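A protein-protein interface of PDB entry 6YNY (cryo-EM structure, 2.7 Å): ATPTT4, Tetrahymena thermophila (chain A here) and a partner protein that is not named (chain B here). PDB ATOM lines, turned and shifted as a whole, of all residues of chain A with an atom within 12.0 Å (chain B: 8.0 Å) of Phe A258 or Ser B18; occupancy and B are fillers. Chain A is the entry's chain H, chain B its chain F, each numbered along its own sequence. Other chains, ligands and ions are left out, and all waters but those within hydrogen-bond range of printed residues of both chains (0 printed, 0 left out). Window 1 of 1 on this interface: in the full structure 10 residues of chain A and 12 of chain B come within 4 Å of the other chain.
O of Lys B15 sits close to NE2 of His B17, 3.4 Å away. The side-chain carboxylate (OD1) of Asp B71 lies close to the backbone NH (N) of Gly B73 (3.3 Å). The side-chain hydroxyl of Ser B18 sits at hydrogen-bond distance from the side-chain carboxylate of Asp B16 (2.6 Å). O of Gln B19 lies close to OG of Ser B22. O of Asp B21 lies within hydrogen-bond range of NH1 of Arg B27 (2.8 Å). OD2 of Asp B71 is in hydrogen-bond range of ND2 of Asn B74, at 3.0 Å.
Printed residues of chain A that touch a printed residue of chain B: Arg A256, Pro A257, Phe A258, Glu A259, His A260, Pro A261, Asn A262 and Pro A263. Hydrophobic or aromatic side chains of chain A that line the printed part of chain B: Pro A257, Phe A258, Pro A261 and Pro A263. Among the printed residues, 22 pairs touch across the chains.
The backbone NH of Phe A258 lies within hydrogen-bond range of the side-chain carboxylate of Asp B21. ND1 of His B17 sits at hydrogen-bond distance from OD1 of Asn A262, at 2.9 Å. The guanidinium group (NH1) of Arg A256 is in salt-bridge range of the side-chain carboxylate (OD1) of Asp B71 (2.9 Å). The backbone carbonyl oxygen (O) of His A260 sits close to the backbone carbonyl oxygen (O) of Asp B16 (3.4 Å). The backbone carbonyl oxygen of His A260 sits close to the backbone carbonyl oxygen of His B17 (2.7 Å). The guanidinium group (NH1) of Arg B27 lies within salt-bridge range of the side-chain carboxylate (OE2) of Glu A259, 3.5 Å away. The backbone carbonyl oxygen of His A260 lies close to the backbone carbonyl oxygen of Ser B18 (3.4 Å). ND2 of Asn B74 sits close to NH2 of Arg A256, at 3.4 Å. NH1 of Arg A256 is in salt-bridge range of OD1 of Asp B21 (3.6 Å).
Among the printed residues, merely in contact across the chains: Arg A256 with Gly B73 (3.6 Å), Pro A257 with Asp B21 (3.0 Å), Pro A257 with Arg B27 (3.4 Å), Phe A258 with Asp B16 (3.0 Å), Phe A258 with Ser B18 (3.4 Å), Phe A258 with Gln B19 (3.8 Å), Phe A258 with Ser B22 (3.7 Å), Glu A259 with Gln B19 (3.6 Å), Glu A259 with Ser B22 (3.999 Å), His A260 with Gln B19 (3.7 Å), Pro A261 with His B17 (3.4 Å), Pro A261 with Gln B19 (3.5 Å) and Pro A263 with His B17 (3.6 Å).
Of the printed residues of chain B, Arg A256 touches Asp B21 (3.3 Å), Asp B71 (2.9 Å), Gly B73 (3.6 Å) and Asn B74 (3.4 Å). Of the printed residues of chain B, Pro A257 touches Asp B21 (3.0 Å) and Arg B27 (3.4 Å). Of the printed residues of chain B, Phe A258 touches Asp B16 (3.0 Å), Ser B18 (3.4 Å), Gln B19 (3.8 Å), Asp B21 (2.5 Å) and Ser B22 (3.7 Å). Of the printed residues of chain B, His A260 touches Asp B16, His B17, Ser B18 and Gln B19. Printed residues of chain B within 4 Å of Asn A262: His B17 (2.9 Å). Of the printed residues of chain A, Asp B16 touches Phe A258 (3.0 Å) and His A260 (3.4 Å). Of chain A, only His A260, Pro A261, Asn A262 and Pro A263 come within 4 Å of His B17. Of chain A, only Phe A258 (3.4 Å) and His A260 (3.4 Å) come within 4 Å of Ser B18. Of chain A, only Phe A258, Glu A259, His A260 and Pro A261 come within 4 Å of Gln B19. No residue of chain A comes within 4 Å of Ala B20. Of the printed residues of chain A, Ser B22 touches Phe A258 and Glu A259. Arg B76 touches none of the printed residues of chain A. Lys B80 touches none of the printed residues of chain A. The nearest printed residue of chain B that does not touch Phe A258 is Gly B73 (4.01 Å). The nearest printed residue of chain B that does not touch Arg A256 is Arg B72 (5.5 Å).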
ATOM      1  N   PHE A 251      22.196  15.418  -7.008  1.00  0.00           N
ATOM      2  CA  PHE A 251      22.003  15.147  -8.425  1.00  0.00           C
ATOM      3  C   PHE A 251      21.922  16.420  -9.252  1.00  0.00           C
ATOM      4  O   PHE A 251      22.016  16.348 -10.482  1.00  0.00           O
ATOM      5  CB  PHE A 251      20.734  14.319  -8.625  1.00  0.00           C
ATOM      6  CG  PHE A 251      19.466  15.073  -8.356  1.00  0.00           C
ATOM      7  CD1 PHE A 251      18.715  15.581  -9.397  1.00  0.00           C
ATOM      8  CD2 PHE A 251      19.021  15.271  -7.065  1.00  0.00           C
ATOM      9  CE1 PHE A 251      17.552  16.269  -9.154  1.00  0.00           C
ATOM     10  CE2 PHE A 251      17.860  15.961  -6.820  1.00  0.00           C
ATOM     11  CZ  PHE A 251      17.125  16.459  -7.866  1.00  0.00           C
ATOM     12  N   LEU A 252      21.754  17.574  -8.611  1.00  0.00           N
ATOM     13  CA  LEU A 252      21.685  18.847  -9.309  1.00  0.00           C
ATOM     14  C   LEU A 252      23.051  19.470  -9.549  1.00  0.00           C
ATOM     15  O   LEU A 252      23.159  20.392 -10.364  1.00  0.00           O
ATOM     16  CB  LEU A 252      20.828  19.832  -8.515  1.00  0.00           C
ATOM     17  CG  LEU A 252      19.389  19.403  -8.264  1.00  0.00           C
ATOM     18  CD1 LEU A 252      18.750  20.289  -7.224  1.00  0.00           C
ATOM     19  CD2 LEU A 252      18.611  19.443  -9.552  1.00  0.00           C
ATOM     20  N   GLU A 253      24.090  18.997  -8.867  1.00  0.00           N
ATOM     21  CA  GLU A 253      25.425  19.577  -8.993  1.00  0.00           C
ATOM     22  C   GLU A 253      26.184  18.957 -10.159  1.00  0.00           C
ATOM     23  O   GLU A 253      27.289  18.436 -10.016  1.00  0.00           O
ATOM     24  CB  GLU A 253      26.189  19.410  -7.688  1.00  0.00           C
ATOM     25  CG  GLU A 253      27.495  20.192  -7.623  1.00  0.00           C
ATOM     26  CD  GLU A 253      27.280  21.682  -7.696  1.00  0.00           C
ATOM     27  OE1 GLU A 253      26.131  22.127  -7.495  1.00  0.00           O
ATOM     28  OE2 GLU A 253      28.261  22.411  -7.959  1.00  0.00           O
ATOM     29  N   GLN A 254      25.568  19.004 -11.331  1.00  0.00           N
ATOM     30  CA  GLN A 254      26.199  18.610 -12.584  1.00  0.00           C
ATOM     31  C   GLN A 254      26.351  19.863 -13.435  1.00  0.00           C
ATOM     32  O   GLN A 254      25.394  20.315 -14.070  1.00  0.00           O
ATOM     33  CB  GLN A 254      25.388  17.540 -13.304  1.00  0.00           C
ATOM     34  CG  GLN A 254      26.125  16.228 -13.455  1.00  0.00           C
ATOM     35  CD  GLN A 254      27.430  16.379 -14.214  1.00  0.00           C
ATOM     36  OE1 GLN A 254      27.750  17.458 -14.712  1.00  0.00           O
ATOM     37  NE2 GLN A 254      28.195  15.300 -14.299  1.00  0.00           N
ATOM     38  N   ARG A 255      27.552  20.423 -13.439  1.00  0.00           N
ATOM     39  CA  ARG A 255      27.843  21.635 -14.178  1.00  0.00           C
ATOM     40  C   ARG A 255      28.574  21.275 -15.463  1.00  0.00           C
ATOM     41  O   ARG A 255      28.771  20.105 -15.794  1.00  0.00           O
ATOM     42  CB  ARG A 255      28.691  22.595 -13.343  1.00  0.00           C
ATOM     43  CG  ARG A 255      28.287  22.749 -11.894  1.00  0.00           C
ATOM     44  CD  ARG A 255      26.888  23.281 -11.737  1.00  0.00           C
ATOM     45  NE  ARG A 255      26.521  23.439 -10.336  1.00  0.00           N
ATOM     46  CZ  ARG A 255      26.874  24.478  -9.587  1.00  0.00           C
ATOM     47  NH1 ARG A 255      27.603  25.453 -10.098  1.00  0.00           N
ATOM     48  NH2 ARG A 255      26.498  24.548  -8.323  1.00  0.00           N
ATOM     49  N   ARG A 256      28.976  22.302 -16.201  1.00  0.00           N
ATOM     50  CA  ARG A 256      29.831  22.084 -17.344  1.00  0.00           C
ATOM     51  C   ARG A 256      31.128  21.420 -16.892  1.00  0.00           C
ATOM     52  O   ARG A 256      31.506  21.512 -15.722  1.00  0.00           O
ATOM     53  CB  ARG A 256      30.133  23.398 -18.046  1.00  0.00           C
ATOM     54  CG  ARG A 256      29.045  23.892 -18.968  1.00  0.00           C
ATOM     55  CD  ARG A 256      29.638  24.428 -20.250  1.00  0.00           C
ATOM     56  NE  ARG A 256      28.929  25.590 -20.752  1.00  0.00           N
ATOM     57  CZ  ARG A 256      29.265  26.236 -21.861  1.00  0.00           C
ATOM     58  NH1 ARG A 256      30.295  25.827 -22.583  1.00  0.00           N
ATOM     59  NH2 ARG A 256      28.571  27.292 -22.246  1.00  0.00           N
ATOM     60  N   PRO A 257      31.839  20.749 -17.807  1.00  0.00           N
ATOM     61  CA  PRO A 257      31.508  20.601 -19.226  1.00  0.00           C
ATOM     62  C   PRO A 257      30.393  19.603 -19.515  1.00  0.00           C
ATOM     63  O   PRO A 257      30.174  18.659 -18.758  1.00  0.00           O
ATOM     64  CB  PRO A 257      32.826  20.123 -19.834  1.00  0.00           C
ATOM     65  CG  PRO A 257      33.513  19.436 -18.740  1.00  0.00           C
ATOM     66  CD  PRO A 257      33.156  20.175 -17.495  1.00  0.00           C
ATOM     67  N   PHE A 258      29.693  19.832 -20.623  1.00  0.00           N
ATOM     68  CA  PHE A 258      28.597  18.972 -21.044  1.00  0.00           C
ATOM     69  C   PHE A 258      29.144  17.776 -21.809  1.00  0.00           C
ATOM     70  O   PHE A 258      29.811  17.940 -22.835  1.00  0.00           O
ATOM     71  CB  PHE A 258      27.618  19.749 -21.917  1.00  0.00           C
ATOM     72  CG  PHE A 258      26.899  20.857 -21.206  1.00  0.00           C
ATOM     73  CD1 PHE A 258      26.418  20.686 -19.924  1.00  0.00           C
ATOM     74  CD2 PHE A 258      26.694  22.068 -21.831  1.00  0.00           C
ATOM     75  CE1 PHE A 258      25.752  21.703 -19.286  1.00  0.00           C
ATOM     76  CE2 PHE A 258      26.031  23.085 -21.196  1.00  0.00           C
ATOM     77  CZ  PHE A 258      25.560  22.901 -19.921  1.00  0.00           C
ATOM     78  N   GLU A 259      28.860  16.574 -21.310  1.00  0.00           N
ATOM     79  CA  GLU A 259      29.345  15.356 -21.939  1.00  0.00           C
ATOM     80  C   GLU A 259      28.297  14.255 -22.013  1.00  0.00           C
ATOM     81  O   GLU A 259      28.620  13.155 -22.468  1.00  0.00           O
ATOM     82  CB  GLU A 259      30.578  14.834 -21.189  1.00  0.00           C
ATOM     83  CG  GLU A 259      31.719  15.831 -21.124  1.00  0.00           C
ATOM     84  CD  GLU A 259      32.895  15.325 -20.317  1.00  0.00           C
ATOM     85  OE1 GLU A 259      32.764  14.263 -19.672  1.00  0.00           O
ATOM     86  OE2 GLU A 259      33.951  15.990 -20.325  1.00  0.00           O
ATOM     87  N   HIS A 260      27.061  14.512 -21.590  1.00  0.00           N
ATOM     88  CA  HIS A 260      25.999  13.516 -21.598  1.00  0.00           C
ATOM     89  C   HIS A 260      25.125  13.690 -22.828  1.00  0.00           C
ATOM     90  O   HIS A 260      24.710  14.819 -23.126  1.00  0.00           O
ATOM     91  CB  HIS A 260      25.146  13.632 -20.340  1.00  0.00           C
ATOM     92  CG  HIS A 260      25.832  13.149 -19.102  1.00  0.00           C
ATOM     93  ND1 HIS A 260      25.503  11.961 -18.487  1.00  0.00           N
ATOM     94  CD2 HIS A 260      26.836  13.687 -18.371  1.00  0.00           C
ATOM     95  CE1 HIS A 260      26.270  11.792 -17.425  1.00  0.00           C
ATOM     96  NE2 HIS A 260      27.088  12.824 -17.333  1.00  0.00           N
ATOM     97  N   PRO A 261      24.820  12.620 -23.566  1.00  0.00           N
ATOM     98  CA  PRO A 261      23.974  12.766 -24.753  1.00  0.00           C
ATOM     99  C   PRO A 261      22.493  12.714 -24.421  1.00  0.00           C
ATOM    100  O   PRO A 261      22.113  12.714 -23.247  1.00  0.00           O
ATOM    101  CB  PRO A 261      24.400  11.578 -25.615  1.00  0.00           C
ATOM    102  CG  PRO A 261      24.717  10.525 -24.615  1.00  0.00           C
ATOM    103  CD  PRO A 261      25.272  11.228 -23.399  1.00  0.00           C
ATOM    104  N   ASN A 262      21.648  12.677 -25.448  1.00  0.00           N
ATOM    105  CA  ASN A 262      20.221  12.546 -25.218  1.00  0.00           C
ATOM    106  C   ASN A 262      19.939  11.289 -24.396  1.00  0.00           C
ATOM    107  O   ASN A 262      20.714  10.328 -24.429  1.00  0.00           O
ATOM    108  CB  ASN A 262      19.464  12.479 -26.540  1.00  0.00           C
ATOM    109  CG  ASN A 262      19.140  13.847 -27.097  1.00  0.00           C
ATOM    110  OD1 ASN A 262      18.838  14.779 -26.356  1.00  0.00           O
ATOM    111  ND2 ASN A 262      19.190  13.971 -28.413  1.00  0.00           N
ATOM    112  N   PRO A 263      18.842  11.270 -23.647  1.00  0.00           N
ATOM    113  CA  PRO A 263      18.490  10.069 -22.888  1.00  0.00           C
ATOM    114  C   PRO A 263      17.935   8.977 -23.785  1.00  0.00           C
ATOM    115  O   PRO A 263      17.197   9.240 -24.739  1.00  0.00           O
ATOM    116  CB  PRO A 263      17.433  10.576 -21.903  1.00  0.00           C
ATOM    117  CG  PRO A 263      16.828  11.730 -22.574  1.00  0.00           C
ATOM    118  CD  PRO A 263      17.902  12.374 -23.389  1.00  0.00           C
ATOM    119  N   THR A 264      18.296   7.741 -23.468  1.00  0.00           N
ATOM    120  CA  THR A 264      17.890   6.595 -24.262  1.00  0.00           C
ATOM    121  C   THR A 264      16.623   5.970 -23.690  1.00  0.00           C
ATOM    122  O   THR A 264      16.323   6.086 -22.501  1.00  0.00           O
ATOM    123  CB  THR A 264      19.005   5.552 -24.323  1.00  0.00           C
ATOM    124  OG1 THR A 264      18.523   4.372 -24.974  1.00  0.00           O
ATOM    125  CG2 THR A 264      19.488   5.197 -22.937  1.00  0.00           C
ATOM    126  N   LYS B  15      18.258  17.211 -17.680  1.00  0.00           N
ATOM    127  CA  LYS B  15      19.693  17.272 -17.882  1.00  0.00           C
ATOM    128  C   LYS B  15      19.997  17.932 -19.217  1.00  0.00           C
ATOM    129  O   LYS B  15      19.135  18.051 -20.090  1.00  0.00           O
ATOM    130  CB  LYS B  15      20.309  15.875 -17.840  1.00  0.00           C
ATOM    131  CG  LYS B  15      20.479  15.313 -16.443  1.00  0.00           C
ATOM    132  CD  LYS B  15      21.540  14.234 -16.413  1.00  0.00           C
ATOM    133  CE  LYS B  15      21.965  13.924 -14.996  1.00  0.00           C
ATOM    134  NZ  LYS B  15      23.198  13.085 -14.958  1.00  0.00           N
ATOM    135  N   ASP B  16      21.245  18.362 -19.366  1.00  0.00           N
ATOM    136  CA  ASP B  16      21.704  18.954 -20.613  1.00  0.00           C
ATOM    137  C   ASP B  16      22.098  17.843 -21.574  1.00  0.00           C
ATOM    138  O   ASP B  16      22.986  17.039 -21.271  1.00  0.00           O
ATOM    139  CB  ASP B  16      22.873  19.900 -20.364  1.00  0.00           C
ATOM    140  CG  ASP B  16      23.291  20.649 -21.612  1.00  0.00           C
ATOM    141  OD1 ASP B  16      23.607  19.996 -22.628  1.00  0.00           O
ATOM    142  OD2 ASP B  16      23.288  21.896 -21.586  1.00  0.00           O
ATOM    143  N   HIS B  17      21.438  17.793 -22.726  1.00  0.00           N
ATOM    144  CA  HIS B  17      21.654  16.714 -23.674  1.00  0.00           C
ATOM    145  C   HIS B  17      22.809  16.990 -24.622  1.00  0.00           C
ATOM    146  O   HIS B  17      23.368  16.046 -25.187  1.00  0.00           O
ATOM    147  CB  HIS B  17      20.384  16.473 -24.482  1.00  0.00           C
ATOM    148  CG  HIS B  17      19.175  16.225 -23.639  1.00  0.00           C
ATOM    149  ND1 HIS B  17      17.893  16.421 -24.102  1.00  0.00           N
ATOM    150  CD2 HIS B  17      19.053  15.798 -22.361  1.00  0.00           C
ATOM    151  CE1 HIS B  17      17.033  16.127 -23.144  1.00  0.00           C
ATOM    152  NE2 HIS B  17      17.711  15.747 -22.078  1.00  0.00           N
ATOM    153  N   SER B  18      23.161  18.254 -24.820  1.00  0.00           N
ATOM    154  CA  SER B  18      24.217  18.596 -25.756  1.00  0.00           C
ATOM    155  C   SER B  18      25.546  18.029 -25.278  1.00  0.00           C
ATOM    156  O   SER B  18      25.794  17.883 -24.078  1.00  0.00           O
ATOM    157  CB  SER B  18      24.328  20.111 -25.917  1.00  0.00           C
ATOM    158  OG  SER B  18      24.860  20.718 -24.754  1.00  0.00           O
ATOM    159  N   GLN B  19      26.399  17.699 -26.235  1.00  0.00           N
ATOM    160  CA  GLN B  19      27.754  17.248 -25.964  1.00  0.00           C
ATOM    161  C   GLN B  19      28.744  18.259 -26.518  1.00  0.00           C
ATOM    162  O   GLN B  19      29.762  17.909 -27.117  1.00  0.00           O
ATOM    163  CB  GLN B  19      27.991  15.865 -26.557  1.00  0.00           C
ATOM    164  CG  GLN B  19      27.078  14.805 -25.997  1.00  0.00           C
ATOM    165  CD  GLN B  19      27.251  13.470 -26.682  1.00  0.00           C
ATOM    166  OE1 GLN B  19      26.939  13.321 -27.863  1.00  0.00           O
ATOM    167  NE2 GLN B  19      27.757  12.490 -25.947  1.00  0.00           N
ATOM    168  N   ALA B  20      28.435  19.541 -26.313  1.00  0.00           N
ATOM    169  CA  ALA B  20      29.234  20.610 -26.892  1.00  0.00           C
ATOM    170  C   ALA B  20      30.680  20.554 -26.431  1.00  0.00           C
ATOM    171  O   ALA B  20      31.589  20.891 -27.197  1.00  0.00           O
ATOM    172  CB  ALA B  20      28.616  21.956 -26.530  1.00  0.00           C
ATOM    173  N   ASP B  21      30.914  20.140 -25.191  1.00  0.00           N
ATOM    174  CA  ASP B  21      32.253  20.131 -24.627  1.00  0.00           C
ATOM    175  C   ASP B  21      33.008  18.842 -24.910  1.00  0.00           C
ATOM    176  O   ASP B  21      34.196  18.753 -24.583  1.00  0.00           O
ATOM    177  CB  ASP B  21      32.183  20.375 -23.120  1.00  0.00           C
ATOM    178  CG  ASP B  21      31.569  21.717 -22.779  1.00  0.00           C
ATOM    179  OD1 ASP B  21      31.915  22.716 -23.443  1.00  0.00           O
ATOM    180  OD2 ASP B  21      30.731  21.776 -21.857  1.00  0.00           O
ATOM    181  N   SER B  22      32.353  17.845 -25.507  1.00  0.00           N
ATOM    182  CA  SER B  22      33.059  16.629 -25.892  1.00  0.00           C
ATOM    183  C   SER B  22      34.171  16.937 -26.882  1.00  0.00           C
ATOM    184  O   SER B  22      35.244  16.323 -26.839  1.00  0.00           O
ATOM    185  CB  SER B  22      32.077  15.621 -26.479  1.00  0.00           C
ATOM    186  OG  SER B  22      31.170  15.169 -25.492  1.00  0.00           O
ATOM    187  N   TRP B  23      33.931  17.881 -27.787  1.00  0.00           N
ATOM    188  CA  TRP B  23      34.959  18.339 -28.710  1.00  0.00           C
ATOM    189  C   TRP B  23      35.926  19.246 -27.962  1.00  0.00           C
ATOM    190  O   TRP B  23      35.513  20.235 -27.350  1.00  0.00           O
ATOM    191  CB  TRP B  23      34.322  19.071 -29.886  1.00  0.00           C
ATOM    192  CG  TRP B  23      35.235  19.266 -31.053  1.00  0.00           C
ATOM    193  CD1 TRP B  23      36.493  18.765 -31.206  1.00  0.00           C
ATOM    194  CD2 TRP B  23      34.958  20.022 -32.237  1.00  0.00           C
ATOM    195  NE1 TRP B  23      37.017  19.162 -32.412  1.00  0.00           N
ATOM    196  CE2 TRP B  23      36.094  19.936 -33.063  1.00  0.00           C
ATOM    197  CE3 TRP B  23      33.858  20.764 -32.677  1.00  0.00           C
ATOM    198  CZ2 TRP B  23      36.163  20.561 -34.303  1.00  0.00           C
ATOM    199  CZ3 TRP B  23      33.929  21.385 -33.907  1.00  0.00           C
ATOM    200  CH2 TRP B  23      35.073  21.280 -34.707  1.00  0.00           C
ATOM    201  N   ARG B  27      36.319  23.929 -27.099  1.00  0.00           N
ATOM    202  CA  ARG B  27      36.067  24.389 -25.741  1.00  0.00           C
ATOM    203  C   ARG B  27      36.437  25.859 -25.600  1.00  0.00           C
ATOM    204  O   ARG B  27      37.487  26.303 -26.071  1.00  0.00           O
ATOM    205  CB  ARG B  27      36.857  23.548 -24.744  1.00  0.00           C
ATOM    206  CG  ARG B  27      36.264  22.183 -24.497  1.00  0.00           C
ATOM    207  CD  ARG B  27      37.231  21.290 -23.754  1.00  0.00           C
ATOM    208  NE  ARG B  27      36.646  19.990 -23.442  1.00  0.00           N
ATOM    209  CZ  ARG B  27      35.994  19.708 -22.320  1.00  0.00           C
ATOM    210  NH1 ARG B  27      35.500  18.492 -22.134  1.00  0.00           N
ATOM    211  NH2 ARG B  27      35.835  20.631 -21.381  1.00  0.00           N
ATOM    212  N   ASP B  71      30.933  29.760 -28.356  1.00  0.00           N
ATOM    213  CA  ASP B  71      30.594  28.895 -27.229  1.00  0.00           C
ATOM    214  C   ASP B  71      29.361  28.081 -27.598  1.00  0.00           C
ATOM    215  O   ASP B  71      28.225  28.522 -27.435  1.00  0.00           O
ATOM    216  CB  ASP B  71      30.372  29.715 -25.967  1.00  0.00           C
ATOM    217  CG  ASP B  71      30.227  28.855 -24.733  1.00  0.00           C
ATOM    218  OD1 ASP B  71      30.377  27.622 -24.847  1.00  0.00           O
ATOM    219  OD2 ASP B  71      29.964  29.411 -23.647  1.00  0.00           O
ATOM    220  N   ARG B  72      29.594  26.869 -28.103  1.00  0.00           N
ATOM    221  CA  ARG B  72      28.495  26.020 -28.540  1.00  0.00           C
ATOM    222  C   ARG B  72      27.608  25.590 -27.381  1.00  0.00           C
ATOM    223  O   ARG B  72      26.462  25.191 -27.608  1.00  0.00           O
ATOM    224  CB  ARG B  72      29.048  24.793 -29.268  1.00  0.00           C
ATOM    225  CG  ARG B  72      29.970  25.139 -30.420  1.00  0.00           C
ATOM    226  CD  ARG B  72      30.431  23.909 -31.191  1.00  0.00           C
ATOM    227  NE  ARG B  72      29.386  23.363 -32.055  1.00  0.00           N
ATOM    228  CZ  ARG B  72      28.557  22.380 -31.715  1.00  0.00           C
ATOM    229  NH1 ARG B  72      27.647  21.963 -32.583  1.00  0.00           N
ATOM    230  NH2 ARG B  72      28.633  21.811 -30.521  1.00  0.00           N
ATOM    231  N   GLY B  73      28.111  25.662 -26.148  1.00  0.00           N
ATOM    232  CA  GLY B  73      27.322  25.288 -24.990  1.00  0.00           C
ATOM    233  C   GLY B  73      26.170  26.222 -24.692  1.00  0.00           C
ATOM    234  O   GLY B  73      25.218  25.815 -24.022  1.00  0.00           O
ATOM    235  N   ASN B  74      26.238  27.463 -25.164  1.00  0.00           N
ATOM    236  CA  ASN B  74      25.180  28.440 -24.953  1.00  0.00           C
ATOM    237  C   ASN B  74      24.121  28.408 -26.043  1.00  0.00           C
ATOM    238  O   ASN B  74      23.239  29.272 -26.057  1.00  0.00           O
ATOM    239  CB  ASN B  74      25.769  29.848 -24.868  1.00  0.00           C
ATOM    240  CG  ASN B  74      25.939  30.324 -23.448  1.00  0.00           C
ATOM    241  OD1 ASN B  74      24.973  30.690 -22.784  1.00  0.00           O
ATOM    242  ND2 ASN B  74      27.175  30.343 -22.980  1.00  0.00           N
ATOM    243  N   LYS B  75      24.182  27.441 -26.949  1.00  0.00           N
ATOM    244  CA  LYS B  75      23.217  27.383 -28.033  1.00  0.00           C
ATOM    245  C   LYS B  75      21.828  27.039 -27.519  1.00  0.00           C
ATOM    246  O   LYS B  75      21.655  26.155 -26.677  1.00  0.00           O
ATOM    247  CB  LYS B  75      23.647  26.354 -29.071  1.00  0.00           C
ATOM    248  CG  LYS B  75      24.696  26.839 -30.033  1.00  0.00           C
ATOM    249  CD  LYS B  75      25.157  25.719 -30.926  1.00  0.00           C
ATOM    250  CE  LYS B  75      26.143  26.200 -31.952  1.00  0.00           C
ATOM    251  NZ  LYS B  75      25.513  27.071 -32.961  1.00  0.00           N
ATOM    252  N   ARG B  76      20.834  27.753 -28.038  1.00  0.00           N
ATOM    253  CA  ARG B  76      19.431  27.469 -27.760  1.00  0.00           C
ATOM    254  C   ARG B  76      19.121  27.595 -26.272  1.00  0.00           C
ATOM    255  O   ARG B  76      18.313  26.846 -25.722  1.00  0.00           O
ATOM    256  CB  ARG B  76      19.054  26.085 -28.283  1.00  0.00           C
ATOM    257  CG  ARG B  76      19.279  25.911 -29.771  1.00  0.00           C
ATOM    258  CD  ARG B  76      19.081  24.477 -30.204  1.00  0.00           C
ATOM    259  NE  ARG B  76      20.075  23.577 -29.628  1.00  0.00           N
ATOM    260  CZ  ARG B  76      21.228  23.254 -30.203  1.00  0.00           C
ATOM    261  NH1 ARG B  76      21.561  23.748 -31.384  1.00  0.00           N
ATOM    262  NH2 ARG B  76      22.055  22.426 -29.587  1.00  0.00           N
ATOM    263  N   LYS B  80      15.416  27.145 -24.121  1.00  0.00           N
ATOM    264  CA  LYS B  80      15.364  26.201 -23.012  1.00  0.00           C
ATOM    265  C   LYS B  80      14.800  26.839 -21.750  1.00  0.00           C
ATOM    266  O   LYS B  80      14.091  26.181 -20.981  1.00  0.00           O
ATOM    267  CB  LYS B  80      16.759  25.644 -22.758  1.00  0.00           C
ATOM    268  CG  LYS B  80      17.226  24.692 -23.827  1.00  0.00           C
ATOM    269  CD  LYS B  80      18.676  24.332 -23.653  1.00  0.00           C
ATOM    270  CE  LYS B  80      19.120  23.354 -24.709  1.00  0.00           C
ATOM    271  NZ  LYS B  80      20.518  22.928 -24.514  1.00  0.00           N
